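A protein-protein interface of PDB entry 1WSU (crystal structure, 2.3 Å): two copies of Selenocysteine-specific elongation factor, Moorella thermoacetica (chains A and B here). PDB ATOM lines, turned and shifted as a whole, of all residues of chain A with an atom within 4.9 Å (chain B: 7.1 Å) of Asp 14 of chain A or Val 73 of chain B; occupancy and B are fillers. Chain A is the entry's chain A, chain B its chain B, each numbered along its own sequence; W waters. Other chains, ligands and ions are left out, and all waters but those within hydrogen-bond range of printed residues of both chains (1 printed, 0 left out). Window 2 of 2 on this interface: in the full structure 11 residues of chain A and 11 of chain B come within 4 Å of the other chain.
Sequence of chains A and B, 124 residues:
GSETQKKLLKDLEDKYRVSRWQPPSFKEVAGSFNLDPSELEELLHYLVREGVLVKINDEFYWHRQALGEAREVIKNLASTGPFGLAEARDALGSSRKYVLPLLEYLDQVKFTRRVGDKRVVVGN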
ATOM      1  N   LYS A  10     -11.544  -1.850 -14.210  1.00  0.00           N
ATOM      2  CA  LYS A  10     -10.690  -2.521 -15.163  1.00  0.00           C
ATOM      3  C   LYS A  10     -11.318  -2.470 -16.557  1.00  0.00           C
ATOM      4  O   LYS A  10     -10.637  -2.230 -17.553  1.00  0.00           O
ATOM      5  CB  LYS A  10     -10.499  -3.972 -14.729  1.00  0.00           C
ATOM      6  CG  LYS A  10      -9.046  -4.421 -14.667  1.00  0.00           C
ATOM      7  CD  LYS A  10      -8.282  -3.782 -13.511  1.00  0.00           C
ATOM      8  CE  LYS A  10      -6.790  -4.114 -13.599  1.00  0.00           C
ATOM      9  NZ  LYS A  10      -6.002  -3.622 -12.437  1.00  0.00           N
ATOM     10  N   ASP A  11     -12.621  -2.681 -16.637  1.00  0.00           N
ATOM     11  CA  ASP A  11     -13.265  -2.658 -17.935  1.00  0.00           C
ATOM     12  C   ASP A  11     -13.317  -1.231 -18.470  1.00  0.00           C
ATOM     13  O   ASP A  11     -13.351  -1.033 -19.688  1.00  0.00           O
ATOM     14  CB  ASP A  11     -14.682  -3.254 -17.867  1.00  0.00           C
ATOM     15  CG  ASP A  11     -14.682  -4.761 -17.571  1.00  0.00           C
ATOM     16  OD1 ASP A  11     -13.672  -5.441 -17.880  1.00  0.00           O
ATOM     17  OD2 ASP A  11     -15.702  -5.268 -17.040  1.00  0.00           O
ATOM     18  N   LEU A  12     -13.325  -0.248 -17.566  1.00  0.00           N
ATOM     19  CA  LEU A  12     -13.376   1.160 -17.962  1.00  0.00           C
ATOM     20  C   LEU A  12     -12.014   1.536 -18.514  1.00  0.00           C
ATOM     21  O   LEU A  12     -11.906   2.141 -19.584  1.00  0.00           O
ATOM     22  CB  LEU A  12     -13.708   2.065 -16.765  1.00  0.00           C
ATOM     23  CG  LEU A  12     -15.153   2.521 -16.591  1.00  0.00           C
ATOM     24  CD1 LEU A  12     -15.379   3.020 -15.173  1.00  0.00           C
ATOM     25  CD2 LEU A  12     -15.446   3.613 -17.611  1.00  0.00           C
ATOM     26  N   GLU A  13     -10.975   1.178 -17.766  1.00  0.00           N
ATOM     27  CA  GLU A  13      -9.625   1.461 -18.189  1.00  0.00           C
ATOM     28  C   GLU A  13      -9.383   0.850 -19.564  1.00  0.00           C
ATOM     29  O   GLU A  13      -8.915   1.529 -20.476  1.00  0.00           O
ATOM     30  CB  GLU A  13      -8.624   0.909 -17.183  1.00  0.00           C
ATOM     31  CG  GLU A  13      -7.233   0.984 -17.705  1.00  0.00           C
ATOM     32  CD  GLU A  13      -6.193   0.850 -16.625  1.00  0.00           C
ATOM     33  OE1 GLU A  13      -6.558   0.631 -15.456  1.00  0.00           O
ATOM     34  OE2 GLU A  13      -4.998   0.968 -16.951  1.00  0.00           O
ATOM     35  N   ASP A  14      -9.727  -0.421 -19.718  1.00  0.00           N
ATOM     36  CA  ASP A  14      -9.545  -1.087 -20.996  1.00  0.00           C
ATOM     37  C   ASP A  14     -10.305  -0.417 -22.125  1.00  0.00           C
ATOM     38  O   ASP A  14      -9.878  -0.460 -23.271  1.00  0.00           O
ATOM     39  CB  ASP A  14      -9.970  -2.558 -20.909  1.00  0.00           C
ATOM     40  CG  ASP A  14      -9.009  -3.381 -20.085  1.00  0.00           C
ATOM     41  OD1 ASP A  14      -7.811  -3.452 -20.443  1.00  0.00           O
ATOM     42  OD2 ASP A  14      -9.445  -3.953 -19.071  1.00  0.00           O
ATOM     43  N   LYS A  15     -11.442   0.185 -21.817  1.00  0.00           N
ATOM     44  CA  LYS A  15     -12.218   0.857 -22.850  1.00  0.00           C
ATOM     45  C   LYS A  15     -11.311   1.957 -23.411  1.00  0.00           C
ATOM     46  O   LYS A  15     -11.214   2.158 -24.622  1.00  0.00           O
ATOM     47  CB  LYS A  15     -13.453   1.502 -22.224  1.00  0.00           C
ATOM     48  CG  LYS A  15     -14.754   1.290 -22.944  1.00  0.00           C
ATOM     49  CD  LYS A  15     -14.777   1.842 -24.325  1.00  0.00           C
ATOM     50  CE  LYS A  15     -16.207   1.751 -24.869  1.00  0.00           C
ATOM     51  NZ  LYS A  15     -16.249   1.906 -26.347  1.00  0.00           N
ATOM     52  N   TYR A  16     -10.631   2.660 -22.512  1.00  0.00           N
ATOM     53  CA  TYR A  16      -9.774   3.757 -22.933  1.00  0.00           C
ATOM     54  C   TYR A  16      -8.445   3.270 -23.498  1.00  0.00           C
ATOM     55  O   TYR A  16      -7.942   3.832 -24.447  1.00  0.00           O
ATOM     56  CB  TYR A  16      -9.544   4.730 -21.770  1.00  0.00           C
ATOM     57  CG  TYR A  16     -10.739   5.610 -21.456  1.00  0.00           C
ATOM     58  CD1 TYR A  16     -11.695   5.240 -20.489  1.00  0.00           C
ATOM     59  CD2 TYR A  16     -10.918   6.822 -22.130  1.00  0.00           C
ATOM     60  CE1 TYR A  16     -12.797   6.068 -20.210  1.00  0.00           C
ATOM     61  CE2 TYR A  16     -12.011   7.648 -21.864  1.00  0.00           C
ATOM     62  CZ  TYR A  16     -12.942   7.268 -20.912  1.00  0.00           C
ATOM     63  OH  TYR A  16     -14.027   8.087 -20.720  1.00  0.00           O
ATOM     64  N   ARG A  17      -7.884   2.222 -22.915  1.00  0.00           N
ATOM     65  CA  ARG A  17      -6.625   1.674 -23.392  1.00  0.00           C
ATOM     66  C   ARG A  17      -6.797   1.182 -24.843  1.00  0.00           C
ATOM     67  O   ARG A  17      -5.992   1.480 -25.720  1.00  0.00           O
ATOM     68  CB  ARG A  17      -6.198   0.539 -22.451  1.00  0.00           C
ATOM     69  CG  ARG A  17      -5.295  -0.529 -23.054  1.00  0.00           C
ATOM     70  CD  ARG A  17      -3.974  -0.655 -22.307  1.00  0.00           C
ATOM     71  NE  ARG A  17      -4.089  -0.827 -20.856  1.00  0.00           N
ATOM     72  CZ  ARG A  17      -3.171  -0.379 -19.995  1.00  0.00           C
ATOM     73  NH1 ARG A  17      -3.317  -0.562 -18.699  1.00  0.00           N
ATOM     74  NH2 ARG A  17      -2.101   0.271 -20.428  1.00  0.00           N
ATOM     75  N   VAL A  18      -7.865   0.445 -25.095  1.00  0.00           N
ATOM     76  CA  VAL A  18      -8.131  -0.066 -26.426  1.00  0.00           C
ATOM     77  C   VAL A  18      -8.437   1.058 -27.398  1.00  0.00           C
ATOM     78  O   VAL A  18      -7.785   1.166 -28.432  1.00  0.00           O
ATOM     79  CB  VAL A  18      -9.286  -1.093 -26.385  1.00  0.00           C
ATOM     80  CG1 VAL A  18      -9.714  -1.495 -27.803  1.00  0.00           C
ATOM     81  CG2 VAL A  18      -8.824  -2.336 -25.599  1.00  0.00           C
ATOM     82  N   SER A  19      -9.406   1.908 -27.065  1.00  0.00           N
ATOM     83  CA  SER A  19      -9.791   3.036 -27.929  1.00  0.00           C
ATOM     84  C   SER A  19      -8.617   3.964 -28.250  1.00  0.00           C
ATOM     85  O   SER A  19      -8.592   4.618 -29.287  1.00  0.00           O
ATOM     86  CB  SER A  19     -10.914   3.828 -27.277  1.00  0.00           C
ATOM     87  OG  SER A  19     -12.118   3.090 -27.325  1.00  0.00           O
ATOM     88  N   ARG B  20       0.482  -0.082 -33.832  1.00  0.00           N
ATOM     89  CA  ARG B  20       0.223  -0.832 -32.614  1.00  0.00           C
ATOM     90  C   ARG B  20      -0.048  -2.319 -32.690  1.00  0.00           C
ATOM     91  O   ARG B  20       0.878  -3.112 -32.732  1.00  0.00           O
ATOM     92  CB  ARG B  20      -0.944  -0.217 -31.808  1.00  0.00           C
ATOM     93  CG  ARG B  20      -0.508   0.553 -30.580  1.00  0.00           C
ATOM     94  CD  ARG B  20      -1.303   0.264 -29.278  1.00  0.00           C
ATOM     95  NE  ARG B  20      -2.749   0.296 -29.430  1.00  0.00           N
ATOM     96  CZ  ARG B  20      -3.617   0.506 -28.435  1.00  0.00           C
ATOM     97  NH1 ARG B  20      -3.219   0.726 -27.176  1.00  0.00           N
ATOM     98  NH2 ARG B  20      -4.911   0.476 -28.705  1.00  0.00           N
ATOM     99  N   TRP B  21      -1.333  -2.680 -32.656  1.00  0.00           N
ATOM    100  CA  TRP B  21      -1.755  -4.076 -32.628  1.00  0.00           C
ATOM    101  C   TRP B  21      -2.031  -4.694 -33.972  1.00  0.00           C
ATOM    102  O   TRP B  21      -2.454  -5.843 -34.061  1.00  0.00           O
ATOM    103  CB  TRP B  21      -2.970  -4.231 -31.710  1.00  0.00           C
ATOM    104  CG  TRP B  21      -2.684  -3.777 -30.318  1.00  0.00           C
ATOM    105  CD1 TRP B  21      -1.449  -3.663 -29.728  1.00  0.00           C
ATOM    106  CD2 TRP B  21      -3.642  -3.413 -29.316  1.00  0.00           C
ATOM    107  NE1 TRP B  21      -1.587  -3.250 -28.419  1.00  0.00           N
ATOM    108  CE2 TRP B  21      -2.924  -3.093 -28.145  1.00  0.00           C
ATOM    109  CE3 TRP B  21      -5.037  -3.338 -29.292  1.00  0.00           C
ATOM    110  CZ2 TRP B  21      -3.558  -2.704 -26.965  1.00  0.00           C
ATOM    111  CZ3 TRP B  21      -5.665  -2.950 -28.119  1.00  0.00           C
ATOM    112  CH2 TRP B  21      -4.925  -2.637 -26.972  1.00  0.00           C
ATOM    113  N   LEU B  67       3.182  -3.860 -27.210  1.00  0.00           N
ATOM    114  CA  LEU B  67       3.191  -5.229 -26.715  1.00  0.00           C
ATOM    115  C   LEU B  67       2.820  -5.198 -25.236  1.00  0.00           C
ATOM    116  O   LEU B  67       2.015  -6.003 -24.770  1.00  0.00           O
ATOM    117  CB  LEU B  67       4.579  -5.849 -26.879  1.00  0.00           C
ATOM    118  CG  LEU B  67       4.817  -7.246 -26.293  1.00  0.00           C
ATOM    119  CD1 LEU B  67       3.912  -8.275 -26.975  1.00  0.00           C
ATOM    120  CD2 LEU B  67       6.270  -7.612 -26.496  1.00  0.00           C
ATOM    121  N   GLY B  68       3.405  -4.254 -24.507  1.00  0.00           N
ATOM    122  CA  GLY B  68       3.112  -4.154 -23.094  1.00  0.00           C
ATOM    123  C   GLY B  68       1.637  -3.889 -22.849  1.00  0.00           C
ATOM    124  O   GLY B  68       1.033  -4.444 -21.936  1.00  0.00           O
ATOM    125  N   GLU B  69       1.044  -3.041 -23.671  1.00  0.00           N
ATOM    126  CA  GLU B  69      -0.354  -2.722 -23.493  1.00  0.00           C
ATOM    127  C   GLU B  69      -1.236  -3.890 -23.866  1.00  0.00           C
ATOM    128  O   GLU B  69      -2.265  -4.099 -23.246  1.00  0.00           O
ATOM    129  CB  GLU B  69      -0.756  -1.503 -24.332  1.00  0.00           C
ATOM    130  CG  GLU B  69      -0.171  -0.199 -23.862  1.00  0.00           C
ATOM    131  CD  GLU B  69      -1.207   0.913 -23.928  1.00  0.00           C
ATOM    132  OE1 GLU B  69      -1.852   1.175 -22.885  1.00  0.00           O
ATOM    133  OE2 GLU B  69      -1.396   1.505 -25.025  1.00  0.00           O
ATOM    134  N   ALA B  70      -0.865  -4.633 -24.901  1.00  0.00           N
ATOM    135  CA  ALA B  70      -1.696  -5.762 -25.295  1.00  0.00           C
ATOM    136  C   ALA B  70      -1.694  -6.772 -24.158  1.00  0.00           C
ATOM    137  O   ALA B  70      -2.705  -7.410 -23.884  1.00  0.00           O
ATOM    138  CB  ALA B  70      -1.172  -6.394 -26.547  1.00  0.00           C
ATOM    139  N   ARG B  71      -0.555  -6.882 -23.483  1.00  0.00           N
ATOM    140  CA  ARG B  71      -0.411  -7.811 -22.379  1.00  0.00           C
ATOM    141  C   ARG B  71      -1.338  -7.424 -21.249  1.00  0.00           C
ATOM    142  O   ARG B  71      -1.954  -8.281 -20.620  1.00  0.00           O
ATOM    143  CB  ARG B  71       1.049  -7.834 -21.900  1.00  0.00           C
ATOM    144  CG  ARG B  71       1.973  -8.612 -22.877  1.00  0.00           C
ATOM    145  CD  ARG B  71       3.438  -8.455 -22.531  1.00  0.00           C
ATOM    146  NE  ARG B  71       3.705  -8.746 -21.128  1.00  0.00           N
ATOM    147  CZ  ARG B  71       4.645  -9.585 -20.707  1.00  0.00           C
ATOM    148  NH1 ARG B  71       4.816  -9.787 -19.407  1.00  0.00           N
ATOM    149  NH2 ARG B  71       5.412 -10.226 -21.586  1.00  0.00           N
ATOM    150  N   GLU B  72      -1.445  -6.121 -21.009  1.00  0.00           N
ATOM    151  CA  GLU B  72      -2.299  -5.611 -19.956  1.00  0.00           C
ATOM    152  C   GLU B  72      -3.740  -5.967 -20.279  1.00  0.00           C
ATOM    153  O   GLU B  72      -4.506  -6.362 -19.403  1.00  0.00           O
ATOM    154  CB  GLU B  72      -2.157  -4.093 -19.842  1.00  0.00           C
ATOM    155  CG  GLU B  72      -2.211  -3.642 -18.411  1.00  0.00           C
ATOM    156  CD  GLU B  72      -0.997  -4.100 -17.638  1.00  0.00           C
ATOM    157  OE1 GLU B  72      -1.061  -4.178 -16.392  1.00  0.00           O
ATOM    158  OE2 GLU B  72       0.034  -4.369 -18.283  1.00  0.00           O
ATOM    159  N   VAL B  73      -4.108  -5.834 -21.545  1.00  0.00           N
ATOM    160  CA  VAL B  73      -5.459  -6.154 -21.950  1.00  0.00           C
ATOM    161  C   VAL B  73      -5.703  -7.644 -21.794  1.00  0.00           C
ATOM    162  O   VAL B  73      -6.782  -8.058 -21.371  1.00  0.00           O
ATOM    163  CB  VAL B  73      -5.715  -5.781 -23.394  1.00  0.00           C
ATOM    164  CG1 VAL B  73      -7.093  -6.273 -23.816  1.00  0.00           C
ATOM    165  CG2 VAL B  73      -5.619  -4.270 -23.561  1.00  0.00           C
ATOM    166  N   ILE B  74      -4.709  -8.457 -22.138  1.00  0.00           N
ATOM    167  CA  ILE B  74      -4.888  -9.897 -22.008  1.00  0.00           C
ATOM    168  C   ILE B  74      -4.963 -10.299 -20.534  1.00  0.00           C
ATOM    169  O   ILE B  74      -5.756 -11.155 -20.160  1.00  0.00           O
ATOM    170  CB  ILE B  74      -3.772 -10.657 -22.759  1.00  0.00           C
ATOM    171  CG1 ILE B  74      -4.033 -10.524 -24.263  1.00  0.00           C
ATOM    172  CG2 ILE B  74      -3.783 -12.148 -22.380  1.00  0.00           C
ATOM    173  CD1 ILE B  74      -2.931 -11.033 -25.144  1.00  0.00           C
ATOM    174  N   LYS B  75      -4.160  -9.660 -19.692  1.00  0.00           N
ATOM    175  CA  LYS B  75      -4.192  -9.958 -18.272  1.00  0.00           C
ATOM    176  C   LYS B  75      -5.621  -9.766 -17.721  1.00  0.00           C
ATOM    177  O   LYS B  75      -6.184 -10.681 -17.124  1.00  0.00           O
ATOM    178  CB  LYS B  75      -3.220  -9.051 -17.541  1.00  0.00           C
ATOM    179  CG  LYS B  75      -3.235  -9.187 -16.042  1.00  0.00           C
ATOM    180  CD  LYS B  75      -2.269  -8.193 -15.382  1.00  0.00           C
ATOM    181  CE  LYS B  75      -0.803  -8.442 -15.765  1.00  0.00           C
ATOM    182  NZ  LYS B  75      -0.478  -8.135 -17.188  1.00  0.00           N
ATOM    183  N   ASN B  76      -6.217  -8.594 -17.938  1.00  0.00           N
ATOM    184  CA  ASN B  76      -7.570  -8.344 -17.446  1.00  0.00           C
ATOM    185  C   ASN B  76      -8.608  -9.285 -18.042  1.00  0.00           C
ATOM    186  O   ASN B  76      -9.607  -9.594 -17.403  1.00  0.00           O
ATOM    187  CB  ASN B  76      -8.001  -6.906 -17.733  1.00  0.00           C
ATOM    188  CG  ASN B  76      -7.202  -5.895 -16.949  1.00  0.00           C
ATOM    189  OD1 ASN B  76      -7.346  -4.688 -17.156  1.00  0.00           O
ATOM    190  ND2 ASN B  76      -6.350  -6.374 -16.038  1.00  0.00           N
ATOM    191  N   LEU B  77      -8.390  -9.717 -19.277  1.00  0.00           N
ATOM    192  CA  LEU B  77      -9.319 -10.631 -19.925  1.00  0.00           C
ATOM    193  C   LEU B  77      -9.263 -12.033 -19.306  1.00  0.00           C
ATOM    194  O   LEU B  77     -10.278 -12.705 -19.169  1.00  0.00           O
ATOM    195  CB  LEU B  77      -9.000 -10.728 -21.408  1.00  0.00           C
ATOM    196  CG  LEU B  77      -9.501 -11.986 -22.102  1.00  0.00           C
ATOM    197  CD1 LEU B  77     -11.020 -11.944 -22.197  1.00  0.00           C
ATOM    198  CD2 LEU B  77      -8.858 -12.079 -23.492  1.00  0.00           C
ATOM    199  N   ALA B  78      -8.077 -12.464 -18.911  1.00  0.00           N
ATOM    200  CA  ALA B  78      -7.919 -13.797 -18.343  1.00  0.00           C
ATOM    201  C   ALA B  78      -8.186 -13.838 -16.856  1.00  0.00           C
ATOM    202  O   ALA B  78      -8.222 -14.912 -16.259  1.00  0.00           O
ATOM    203  CB  ALA B  78      -6.514 -14.311 -18.620  1.00  0.00           C
ATOM    204  N   SER B  79      -8.377 -12.670 -16.257  1.00  0.00           N
ATOM    205  CA  SER B  79      -8.603 -12.602 -14.830  1.00  0.00           C
ATOM    206  C   SER B  79      -9.836 -13.400 -14.440  1.00  0.00           C
ATOM    207  O   SER B  79      -9.919 -13.886 -13.322  1.00  0.00           O
ATOM    208  CB  SER B  79      -8.787 -11.157 -14.389  1.00  0.00           C
ATOM    209  OG  SER B  79     -10.103 -10.751 -14.697  1.00  0.00           O
ATOM    210  N   ALA B  88      -9.762 -13.064 -27.280  1.00  0.00           N
ATOM    211  CA  ALA B  88      -8.586 -12.210 -27.261  1.00  0.00           C
ATOM    212  C   ALA B  88      -8.695 -11.164 -28.366  1.00  0.00           C
ATOM    213  O   ALA B  88      -8.360  -9.998 -28.169  1.00  0.00           O
ATOM    214  CB  ALA B  88      -7.344 -13.038 -27.462  1.00  0.00           C
ATOM    215  N   ASP B  90     -11.490 -10.038 -29.732  1.00  0.00           N
ATOM    216  CA  ASP B  90     -12.504  -9.062 -29.321  1.00  0.00           C
ATOM    217  C   ASP B  90     -11.954  -8.041 -28.310  1.00  0.00           C
ATOM    218  O   ASP B  90     -12.108  -6.839 -28.490  1.00  0.00           O
ATOM    219  CB  ASP B  90     -13.721  -9.763 -28.694  1.00  0.00           C
ATOM    220  CG  ASP B  90     -14.522 -10.577 -29.697  1.00  0.00           C
ATOM    221  OD1 ASP B  90     -14.330 -10.395 -30.922  1.00  0.00           O
ATOM    222  OD2 ASP B  90     -15.359 -11.396 -29.253  1.00  0.00           O
ATOM    223  N   ALA B  91     -11.322  -8.528 -27.241  1.00  0.00           N
ATOM    224  CA  ALA B  91     -10.762  -7.650 -26.217  1.00  0.00           C
ATOM    225  C   ALA B  91      -9.763  -6.624 -26.754  1.00  0.00           C
ATOM    226  O   ALA B  91      -9.630  -5.536 -26.200  1.00  0.00           O
ATOM    227  CB  ALA B  91     -10.087  -8.475 -25.151  1.00  0.00           C
ATOM    228  N   LEU B  92      -9.059  -6.987 -27.824  1.00  0.00           N
ATOM    229  CA  LEU B  92      -8.046  -6.131 -28.412  1.00  0.00           C
ATOM    230  C   LEU B  92      -8.579  -5.380 -29.615  1.00  0.00           C
ATOM    231  O   LEU B  92      -7.905  -4.505 -30.149  1.00  0.00           O
ATOM    232  CB  LEU B  92      -6.842  -6.966 -28.852  1.00  0.00           C
ATOM    233  CG  LEU B  92      -5.987  -7.718 -27.834  1.00  0.00           C
ATOM    234  CD1 LEU B  92      -5.119  -8.719 -28.578  1.00  0.00           C
ATOM    235  CD2 LEU B  92      -5.131  -6.754 -27.034  1.00  0.00           C
ATOM    236  N   GLY B  93      -9.786  -5.727 -30.040  1.00  0.00           N
ATOM    237  CA  GLY B  93     -10.364  -5.074 -31.202  1.00  0.00           C
ATOM    238  C   GLY B  93      -9.504  -5.287 -32.440  1.00  0.00           C
ATOM    239  O   GLY B  93      -9.409  -4.417 -33.294  1.00  0.00           O
HETATM  240  O   HOH W   1       0.276   0.625 -21.255  1.00  0.00           O
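OD2 of Asp 14 of chain A sits close to OD1 of Asn 76 of chain B (2.9 Å). The backbone carbonyl oxygen (O) of Arg 17 of chain A is in hydrogen-bond range of the guanidinium group (NH1) of Arg 20 of chain B (3.2 Å). OE1 of Glu 69 of chain B is in salt-bridge range of NH2 of Arg 17 of chain A, at 2.6 Å. O of Val 18 of chain A is in hydrogen-bond range of NH2 of Arg 20 of chain B (3.0 Å).
The side-chain carboxylate (OD2) of Asp 14 of chain A sits close to the backbone carbonyl oxygen (O) of Lys 10 of chain A (2.6 Å). The guanidinium group of Arg 17 of chain A lies within salt-bridge range of the side-chain carboxylate of Glu 13 of chain A. The guanidinium group (NH1) of Arg 20 of chain B lies within salt-bridge range of the side-chain carboxylate (OE2) of Glu 69 of chain B, at 2.9 Å. The side-chain amino group (NZ) of Lys 75 of chain B is in salt-bridge range of the side-chain carboxylate (OE2) of Glu 72 of chain B. The backbone carbonyl oxygen (O) of Asn 76 of chain B is in hydrogen-bond range of the side-chain hydroxyl (OG) of Ser 79 of chain B.
CG of Lys 10 of chain A touches OD1 of Asn 76 of chain B, at 3.0 Å. Asp 14 of chain A touches Val 73 of chain B (OD1 to CA, 3.9 Å). CG of Glu 72 of chain B touches NH1 of Arg 17 of chain A, 3.3 Å away. Arg 17 of chain A touches Val 73 of chain B. CG2 of Val 18 of chain A touches O of Ala 91 of chain B, 3.4 Å away.
Of the printed residues of chain B, Asp 14 of chain A touches Val 73 and Asn 76. Val 73 of chain B touches two residues of chain A. Printed residues of chain A within 4 Å of Ala 91 of chain B: Val 18. Printed residues of chain A within 4 Å of Glu 69 of chain B: Arg 17. Printed residues of chain B within 4 Å of Lys 10 of chain A: Asn 76.
Of the 10 printed residues of chain A, 4 touch a printed residue of chain B. Hydrophobic or aromatic side chains of chain A that line the printed part of chain B: Val 18. Along chain A the printed residues that touch a printed residue of chain B span positions 10 to 18. Of the 20 printed residues of chain B, 6 touch a printed residue of chain A. Printed residues of chain B that touch a printed residue of chain A: Arg 20, Glu 69, Glu 72, Val 73, Asn 76 and Ala 91. Hydrophobic or aromatic side chains of chain B within 4 Å of the printed part of chain A: Val 73.
No position is printed for both chains. Of the 9 pairs that touch across the chains among the printed residues, none has its exchanged pair printed and touching as well.
Water W1 lies within hydrogen-bond range of NH2 of Arg 17 of chain A and OE1 of Glu 69 of chain B.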
